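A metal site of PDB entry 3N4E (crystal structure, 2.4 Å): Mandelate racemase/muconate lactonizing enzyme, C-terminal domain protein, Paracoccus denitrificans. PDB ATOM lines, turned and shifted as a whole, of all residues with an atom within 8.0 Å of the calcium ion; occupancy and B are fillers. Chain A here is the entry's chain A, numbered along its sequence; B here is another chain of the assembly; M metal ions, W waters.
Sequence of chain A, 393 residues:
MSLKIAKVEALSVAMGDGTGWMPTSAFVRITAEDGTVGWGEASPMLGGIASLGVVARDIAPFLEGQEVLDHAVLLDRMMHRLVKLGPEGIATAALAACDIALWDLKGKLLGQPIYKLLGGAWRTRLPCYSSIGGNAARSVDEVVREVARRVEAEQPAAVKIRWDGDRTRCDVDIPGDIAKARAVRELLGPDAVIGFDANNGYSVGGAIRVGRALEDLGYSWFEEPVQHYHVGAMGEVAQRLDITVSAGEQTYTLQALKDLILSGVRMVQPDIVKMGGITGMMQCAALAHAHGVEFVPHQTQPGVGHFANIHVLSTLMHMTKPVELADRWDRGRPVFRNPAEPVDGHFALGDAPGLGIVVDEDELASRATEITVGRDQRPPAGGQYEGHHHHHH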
ATOM      1  N   TYR A 129      15.156  17.204   3.477  1.00  0.00           N
ATOM      2  CA  TYR A 129      15.186  18.308   2.531  1.00  0.00           C
ATOM      3  C   TYR A 129      16.280  19.297   2.940  1.00  0.00           C
ATOM      4  O   TYR A 129      16.559  19.469   4.122  1.00  0.00           O
ATOM      5  CB  TYR A 129      13.798  18.945   2.335  1.00  0.00           C
ATOM      6  CG  TYR A 129      13.254  19.899   3.402  1.00  0.00           C
ATOM      7  CD1 TYR A 129      13.652  21.248   3.440  1.00  0.00           C
ATOM      8  CD2 TYR A 129      12.281  19.483   4.320  1.00  0.00           C
ATOM      9  CE1 TYR A 129      13.140  22.129   4.391  1.00  0.00           C
ATOM     10  CE2 TYR A 129      11.757  20.376   5.275  1.00  0.00           C
ATOM     11  CZ  TYR A 129      12.182  21.691   5.296  1.00  0.00           C
ATOM     12  OH  TYR A 129      11.663  22.583   6.242  1.00  0.00           O
ATOM     13  N   SER A 131      17.562  22.696   3.771  1.00  0.00           N
ATOM     14  CA  SER A 131      17.053  23.985   4.217  1.00  0.00           C
ATOM     15  C   SER A 131      18.215  25.000   4.175  1.00  0.00           C
ATOM     16  O   SER A 131      19.151  24.942   4.982  1.00  0.00           O
ATOM     17  CB  SER A 131      16.461  23.844   5.623  1.00  0.00           C
ATOM     18  OG  SER A 131      15.760  24.998   6.023  1.00  0.00           O
ATOM     19  N   LYS A 160      14.378  23.752   0.268  1.00  0.00           N
ATOM     20  CA  LYS A 160      13.754  24.991   0.730  1.00  0.00           C
ATOM     21  C   LYS A 160      14.800  26.103   0.833  1.00  0.00           C
ATOM     22  O   LYS A 160      15.796  25.987   1.541  1.00  0.00           O
ATOM     23  CB  LYS A 160      13.049  24.782   2.062  1.00  0.00           C
ATOM     24  CG  LYS A 160      12.361  26.039   2.614  1.00  0.00           C
ATOM     25  CD  LYS A 160      11.606  25.760   3.886  1.00  0.00           C
ATOM     26  CE  LYS A 160      12.507  25.813   5.120  1.00  0.00           C
ATOM     27  NZ  LYS A 160      11.821  25.189   6.294  1.00  0.00           N
ATOM     28  N   ARG A 162      15.567  29.796   2.083  1.00  0.00           N
ATOM     29  CA  ARG A 162      15.062  30.714   3.094  1.00  0.00           C
ATOM     30  C   ARG A 162      15.738  32.059   2.948  1.00  0.00           C
ATOM     31  O   ARG A 162      16.868  32.141   2.474  1.00  0.00           O
ATOM     32  CB  ARG A 162      15.301  30.180   4.522  1.00  0.00           C
ATOM     33  CG  ARG A 162      15.125  28.656   4.722  1.00  0.00           C
ATOM     34  CD  ARG A 162      15.106  28.301   6.206  1.00  0.00           C
ATOM     35  NE  ARG A 162      16.207  28.981   6.886  1.00  0.00           N
ATOM     36  CZ  ARG A 162      17.428  28.468   7.067  1.00  0.00           C
ATOM     37  NH1 ARG A 162      17.699  27.233   6.639  1.00  0.00           N
ATOM     38  NH2 ARG A 162      18.369  29.192   7.672  1.00  0.00           N
ATOM     39  N   TRP A 163      15.058  33.116   3.378  1.00  0.00           N
ATOM     40  CA  TRP A 163      15.559  34.477   3.174  1.00  0.00           C
ATOM     41  C   TRP A 163      16.337  35.054   4.344  1.00  0.00           C
ATOM     42  O   TRP A 163      17.373  35.673   4.115  1.00  0.00           O
ATOM     43  CB  TRP A 163      14.423  35.423   2.733  1.00  0.00           C
ATOM     44  CG  TRP A 163      14.491  35.737   1.270  1.00  0.00           C
ATOM     45  CD1 TRP A 163      14.571  36.978   0.717  1.00  0.00           C
ATOM     46  CD2 TRP A 163      14.560  34.802   0.186  1.00  0.00           C
ATOM     47  NE1 TRP A 163      14.648  36.869  -0.653  1.00  0.00           N
ATOM     48  CE2 TRP A 163      14.642  35.551  -1.008  1.00  0.00           C
ATOM     49  CE3 TRP A 163      14.534  33.395   0.106  1.00  0.00           C
ATOM     50  CZ2 TRP A 163      14.711  34.941  -2.289  1.00  0.00           C
ATOM     51  CZ3 TRP A 163      14.603  32.794  -1.153  1.00  0.00           C
ATOM     52  CH2 TRP A 163      14.685  33.573  -2.337  1.00  0.00           C
ATOM     53  N   ASP A 164      15.861  34.857   5.579  1.00  0.00           N
ATOM     54  CA  ASP A 164      16.514  35.374   6.796  1.00  0.00           C
ATOM     55  C   ASP A 164      16.749  36.881   6.726  1.00  0.00           C
ATOM     56  O   ASP A 164      17.832  37.376   7.058  1.00  0.00           O
ATOM     57  CB  ASP A 164      17.830  34.624   7.109  1.00  0.00           C
ATOM     58  CG  ASP A 164      17.619  33.116   7.334  1.00  0.00           C
ATOM     59  OD1 ASP A 164      16.864  32.720   8.253  1.00  0.00           O
ATOM     60  OD2 ASP A 164      18.231  32.319   6.600  1.00  0.00           O
ATOM     61  N   PHE A 196       9.825  27.817  -0.390  1.00  0.00           N
ATOM     62  CA  PHE A 196      10.287  29.173  -0.337  1.00  0.00           C
ATOM     63  C   PHE A 196       9.915  29.694   1.038  1.00  0.00           C
ATOM     64  O   PHE A 196       8.748  29.694   1.426  1.00  0.00           O
ATOM     65  CB  PHE A 196       9.624  30.007  -1.434  1.00  0.00           C
ATOM     66  CG  PHE A 196      10.109  31.437  -1.512  1.00  0.00           C
ATOM     67  CD1 PHE A 196       9.688  32.383  -0.570  1.00  0.00           C
ATOM     68  CD2 PHE A 196      10.967  31.848  -2.534  1.00  0.00           C
ATOM     69  CE1 PHE A 196      10.145  33.715  -0.635  1.00  0.00           C
ATOM     70  CE2 PHE A 196      11.408  33.164  -2.619  1.00  0.00           C
ATOM     71  CZ  PHE A 196      11.002  34.096  -1.667  1.00  0.00           C
ATOM     72  N   ASP A 197      10.935  30.122   1.780  1.00  0.00           N
ATOM     73  CA  ASP A 197      10.737  30.549   3.149  1.00  0.00           C
ATOM     74  C   ASP A 197      10.997  32.046   3.211  1.00  0.00           C
ATOM     75  O   ASP A 197      12.134  32.505   3.169  1.00  0.00           O
ATOM     76  CB  ASP A 197      11.653  29.785   4.111  1.00  0.00           C
ATOM     77  CG  ASP A 197      11.376  30.122   5.578  1.00  0.00           C
ATOM     78  OD1 ASP A 197      10.650  31.101   5.881  1.00  0.00           O
ATOM     79  OD2 ASP A 197      11.901  29.405   6.455  1.00  0.00           O
ATOM     80  N   ALA A 198       9.909  32.808   3.289  1.00  0.00           N
ATOM     81  CA  ALA A 198       9.970  34.273   3.294  1.00  0.00           C
ATOM     82  C   ALA A 198      10.499  34.820   4.609  1.00  0.00           C
ATOM     83  O   ALA A 198      10.853  36.003   4.679  1.00  0.00           O
ATOM     84  CB  ALA A 198       8.596  34.861   2.980  1.00  0.00           C
ATOM     85  N   ASN A 199      10.549  33.982   5.654  1.00  0.00           N
ATOM     86  CA  ASN A 199      10.946  34.409   7.005  1.00  0.00           C
ATOM     87  C   ASN A 199      10.322  35.722   7.415  1.00  0.00           C
ATOM     88  O   ASN A 199      11.035  36.661   7.787  1.00  0.00           O
ATOM     89  CB  ASN A 199      12.466  34.566   7.108  1.00  0.00           C
ATOM     90  CG  ASN A 199      13.198  33.237   7.102  1.00  0.00           C
ATOM     91  OD1 ASN A 199      13.936  32.944   6.163  1.00  0.00           O
ATOM     92  ND2 ASN A 199      12.994  32.426   8.145  1.00  0.00           N
ATOM     93  N   ASN A 200       8.993  35.794   7.294  1.00  0.00           N
ATOM     94  CA  ASN A 200       8.212  36.953   7.692  1.00  0.00           C
ATOM     95  C   ASN A 200       8.404  38.236   6.853  1.00  0.00           C
ATOM     96  O   ASN A 200       8.153  39.332   7.338  1.00  0.00           O
ATOM     97  CB  ASN A 200       8.415  37.238   9.193  1.00  0.00           C
ATOM     98  CG  ASN A 200       8.373  35.987  10.049  1.00  0.00           C
ATOM     99  OD1 ASN A 200       9.414  35.518  10.482  1.00  0.00           O
ATOM    100  ND2 ASN A 200       7.181  35.429  10.263  1.00  0.00           N
ATOM    101  N   TRP A 221       5.583  24.675  -1.337  1.00  0.00           N
ATOM    102  CA  TRP A 221       5.069  25.436  -0.192  1.00  0.00           C
ATOM    103  C   TRP A 221       5.753  26.775   0.017  1.00  0.00           C
ATOM    104  O   TRP A 221       6.832  27.021  -0.511  1.00  0.00           O
ATOM    105  CB  TRP A 221       5.069  24.597   1.091  1.00  0.00           C
ATOM    106  CG  TRP A 221       6.376  24.472   1.834  1.00  0.00           C
ATOM    107  CD1 TRP A 221       6.770  25.197   2.905  1.00  0.00           C
ATOM    108  CD2 TRP A 221       7.430  23.530   1.572  1.00  0.00           C
ATOM    109  NE1 TRP A 221       8.001  24.772   3.354  1.00  0.00           N
ATOM    110  CE2 TRP A 221       8.435  23.757   2.541  1.00  0.00           C
ATOM    111  CE3 TRP A 221       7.629  22.515   0.619  1.00  0.00           C
ATOM    112  CZ2 TRP A 221       9.611  23.004   2.596  1.00  0.00           C
ATOM    113  CZ3 TRP A 221       8.791  21.763   0.676  1.00  0.00           C
ATOM    114  CH2 TRP A 221       9.773  22.015   1.653  1.00  0.00           C
ATOM    115  N   GLU A 223       6.599  29.419   3.068  1.00  0.00           N
ATOM    116  CA  GLU A 223       6.765  29.366   4.512  1.00  0.00           C
ATOM    117  C   GLU A 223       6.848  30.761   5.118  1.00  0.00           C
ATOM    118  O   GLU A 223       7.581  31.621   4.631  1.00  0.00           O
ATOM    119  CB  GLU A 223       7.998  28.508   4.865  1.00  0.00           C
ATOM    120  CG  GLU A 223       8.291  28.307   6.360  1.00  0.00           C
ATOM    121  CD  GLU A 223       9.298  27.169   6.633  1.00  0.00           C
ATOM    122  OE1 GLU A 223       9.175  26.076   6.041  1.00  0.00           O
ATOM    123  OE2 GLU A 223      10.229  27.385   7.465  1.00  0.00           O
ATOM    124  N   GLU A 224       6.076  30.973   6.182  1.00  0.00           N
ATOM    125  CA  GLU A 224       5.998  32.261   6.897  1.00  0.00           C
ATOM    126  C   GLU A 224       5.976  33.486   5.981  1.00  0.00           C
ATOM    127  O   GLU A 224       6.882  34.322   6.020  1.00  0.00           O
ATOM    128  CB  GLU A 224       7.114  32.362   7.953  1.00  0.00           C
ATOM    129  CG  GLU A 224       6.927  31.420   9.155  1.00  0.00           C
ATOM    130  CD  GLU A 224       7.658  31.880  10.400  1.00  0.00           C
ATOM    131  OE1 GLU A 224       8.917  31.856  10.418  1.00  0.00           O
ATOM    132  OE2 GLU A 224       6.986  32.271  11.383  1.00  0.00           O
ATOM    133  N   SER A 246       2.804  27.603   4.873  1.00  0.00           N
ATOM    134  CA  SER A 246       3.150  26.944   6.140  1.00  0.00           C
ATOM    135  C   SER A 246       3.666  27.901   7.210  1.00  0.00           C
ATOM    136  O   SER A 246       4.309  28.913   6.904  1.00  0.00           O
ATOM    137  CB  SER A 246       4.180  25.833   5.899  1.00  0.00           C
ATOM    138  OG  SER A 246       5.470  26.364   5.652  1.00  0.00           O
ATOM    139  N   ALA A 247       3.369  27.598   8.466  1.00  0.00           N
ATOM    140  CA  ALA A 247       3.783  28.429   9.600  1.00  0.00           C
ATOM    141  C   ALA A 247       3.777  27.533  10.814  1.00  0.00           C
ATOM    142  O   ALA A 247       3.350  26.385  10.721  1.00  0.00           O
ATOM    143  CB  ALA A 247       2.804  29.602   9.820  1.00  0.00           C
ATOM    144  N   GLU A 249       6.573  27.541  13.299  1.00  0.00           N
ATOM    145  CA  GLU A 249       7.880  27.471  13.944  1.00  0.00           C
ATOM    146  C   GLU A 249       7.965  28.454  15.104  1.00  0.00           C
ATOM    147  O   GLU A 249       8.686  28.196  16.055  1.00  0.00           O
ATOM    148  CB  GLU A 249       9.043  27.640  12.959  1.00  0.00           C
ATOM    149  CG  GLU A 249       9.238  29.024  12.348  1.00  0.00           C
ATOM    150  CD  GLU A 249      10.273  29.019  11.239  1.00  0.00           C
ATOM    151  OE1 GLU A 249      11.361  29.632  11.391  1.00  0.00           O
ATOM    152  OE2 GLU A 249      10.027  28.387  10.192  1.00  0.00           O
ATOM    153  N   GLN A 250       7.207  29.548  15.031  1.00  0.00           N
ATOM    154  CA  GLN A 250       7.146  30.542  16.103  1.00  0.00           C
ATOM    155  C   GLN A 250       5.788  30.493  16.824  1.00  0.00           C
ATOM    156  O   GLN A 250       5.250  31.523  17.247  1.00  0.00           O
ATOM    157  CB  GLN A 250       7.408  31.952  15.566  1.00  0.00           C
ATOM    158  CG  GLN A 250       8.573  32.059  14.597  1.00  0.00           C
ATOM    159  CD  GLN A 250       8.912  33.496  14.255  1.00  0.00           C
ATOM    160  OE1 GLN A 250       9.208  34.309  15.145  1.00  0.00           O
ATOM    161  NE2 GLN A 250       8.861  33.826  12.953  1.00  0.00           N
ATOM    162  N   GLN A 269       4.220  23.740  11.565  1.00  0.00           N
ATOM    163  CA  GLN A 269       5.630  23.447  11.728  1.00  0.00           C
ATOM    164  C   GLN A 269       6.190  23.761  13.125  1.00  0.00           C
ATOM    165  O   GLN A 269       7.243  24.422  13.252  1.00  0.00           O
ATOM    166  CB  GLN A 269       6.408  24.241  10.678  1.00  0.00           C
ATOM    167  CG  GLN A 269       5.792  24.203   9.275  1.00  0.00           C
ATOM    168  CD  GLN A 269       6.649  24.900   8.256  1.00  0.00           C
ATOM    169  OE1 GLN A 269       6.606  26.125   8.133  1.00  0.00           O
ATOM    170  NE2 GLN A 269       7.457  24.136   7.543  1.00  0.00           N
ATOM    171  N   HIS A 298       9.565  22.185  12.217  1.00  0.00           N
ATOM    172  CA  HIS A 298      10.792  22.959  12.043  1.00  0.00           C
ATOM    173  C   HIS A 298      11.866  22.342  12.914  1.00  0.00           C
ATOM    174  O   HIS A 298      11.583  21.920  14.047  1.00  0.00           O
ATOM    175  CB  HIS A 298      10.514  24.410  12.441  1.00  0.00           C
ATOM    176  CG  HIS A 298      11.734  25.276  12.525  1.00  0.00           C
ATOM    177  ND1 HIS A 298      12.515  25.356  13.651  1.00  0.00           N
ATOM    178  CD2 HIS A 298      12.278  26.129  11.623  1.00  0.00           C
ATOM    179  CE1 HIS A 298      13.503  26.207  13.446  1.00  0.00           C
ATOM    180  NE2 HIS A 298      13.389  26.688  12.224  1.00  0.00           N
ATOM    181  N   GLN A 299      13.077  22.248  12.384  1.00  0.00           N
ATOM    182  CA  GLN A 299      14.227  21.735  13.129  1.00  0.00           C
ATOM    183  C   GLN A 299      15.514  22.161  12.480  1.00  0.00           C
ATOM    184  O   GLN A 299      15.729  21.896  11.296  1.00  0.00           O
ATOM    185  CB  GLN A 299      14.214  20.215  13.240  1.00  0.00           C
ATOM    186  CG  GLN A 299      15.418  19.648  14.034  1.00  0.00           C
ATOM    187  CD  GLN A 299      15.445  20.194  15.447  1.00  0.00           C
ATOM    188  OE1 GLN A 299      16.460  20.726  15.922  1.00  0.00           O
ATOM    189  NE2 GLN A 299      14.290  20.109  16.116  1.00  0.00           N
ATOM    190  N   THR A 300      16.366  22.823  13.268  1.00  0.00           N
ATOM    191  CA  THR A 300      17.651  23.295  12.755  1.00  0.00           C
ATOM    192  C   THR A 300      18.870  22.767  13.519  1.00  0.00           C
ATOM    193  O   THR A 300      20.004  23.078  13.159  1.00  0.00           O
ATOM    194  CB  THR A 300      17.703  24.835  12.724  1.00  0.00           C
ATOM    195  OG1 THR A 300      17.426  25.350  14.039  1.00  0.00           O
ATOM    196  CG2 THR A 300      16.698  25.403  11.723  1.00  0.00           C
ATOM    197  N   GLU A 324      13.528  18.385   7.837  1.00  0.00           N
ATOM    198  CA  GLU A 324      14.339  19.575   7.631  1.00  0.00           C
ATOM    199  C   GLU A 324      15.810  19.343   7.989  1.00  0.00           C
ATOM    200  O   GLU A 324      16.130  18.829   9.078  1.00  0.00           O
ATOM    201  CB  GLU A 324      13.788  20.776   8.408  1.00  0.00           C
ATOM    202  CG  GLU A 324      14.500  22.092   8.076  1.00  0.00           C
ATOM    203  CD  GLU A 324      13.841  23.343   8.656  1.00  0.00           C
ATOM    204  OE1 GLU A 324      13.067  23.233   9.649  1.00  0.00           O
ATOM    205  OE2 GLU A 324      14.103  24.446   8.129  1.00  0.00           O
ATOM    206  N   LYS B  84      12.586  35.690  18.699  1.00  0.00           N
ATOM    207  CA  LYS B  84      12.666  34.242  18.859  1.00  0.00           C
ATOM    208  C   LYS B  84      12.801  33.878  20.342  1.00  0.00           C
ATOM    209  O   LYS B  84      12.754  32.701  20.688  1.00  0.00           O
ATOM    210  CB  LYS B  84      13.770  33.602  18.000  1.00  0.00           C
ATOM    211  CG  LYS B  84      13.648  33.802  16.478  1.00  0.00           C
ATOM    212  CD  LYS B  84      12.932  32.675  15.733  1.00  0.00           C
ATOM    213  CE  LYS B  84      13.151  32.820  14.220  1.00  0.00           C
ATOM    214  NZ  LYS B  84      12.600  31.698  13.363  1.00  0.00           N
HETATM  215 CA    CA M   1      11.605  28.790   8.573  1.00  0.00          CA
HETATM  216  O   HOH W   1      10.101  30.513   8.500  1.00  0.00           O
HETATM  217  O   HOH W   2      14.065  29.488   9.725  1.00  0.00           O
HETATM  218  O   HOH W   3      13.403  26.840   8.827  1.00  0.00           O
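The side-chain carboxylate (OD1) of Asp 197 lies within hydrogen-bond range of the backbone NH (N) of Asn 199 (2.9 Å).
N of Trp 163 sits at hydrogen-bond distance from OD1 of Asn 199, 3.0 Å away.
The backbone NH of Glu 223 is in hydrogen-bond range of the backbone carbonyl oxygen of Phe 196 (2.7 Å).
O of Glu 223 lies within hydrogen-bond range of N of Ala 198 (2.9 Å).
O of Gln 269 sits close to N of Glu 249, 3.2 Å away.
OE1 of Glu 223 sits at hydrogen-bond distance from NE2 of Gln 269.
The backbone NH (N) of Trp 163 lies within hydrogen-bond range of the backbone carbonyl oxygen (O) of Asp 197.
The side-chain carboxylate of Glu 223 is in hydrogen-bond range of the indole nitrogen of Trp 221, 3.2 Å away.
Merely in contact with the calcium ion: Asn 199.
Of the 24 residues printed, 4 come within 4 Å of the calcium ion.
Along chain A the residues within 4 Å of the calcium ion span positions 197 to 249.
The calcium ion is bound by the side-chain carboxylate (OD2) of Asp 197 (2.2 Å), the side-chain carboxylate (OE2) of Glu 223 (2.3 Å), water W1 (2.3 Å), the side-chain carboxylate (OE2) of Glu 249 (2.3 Å), water W3 (2.7 Å) and water W2 (2.8 Å).
The calcium ion has six donor atoms within binding distance.
Slightly farther from the calcium ion lies the side-chain carboxylate (OE1) of Glu 249 (3.0 Å).
Water W3 lies within hydrogen-bond range of the side-chain carboxylate of Glu 324 (2.6 Å), a ring nitrogen (NE2) of His 298 (3.4 Å) and the side-chain amino group of Lys 160 (3.4 Å).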
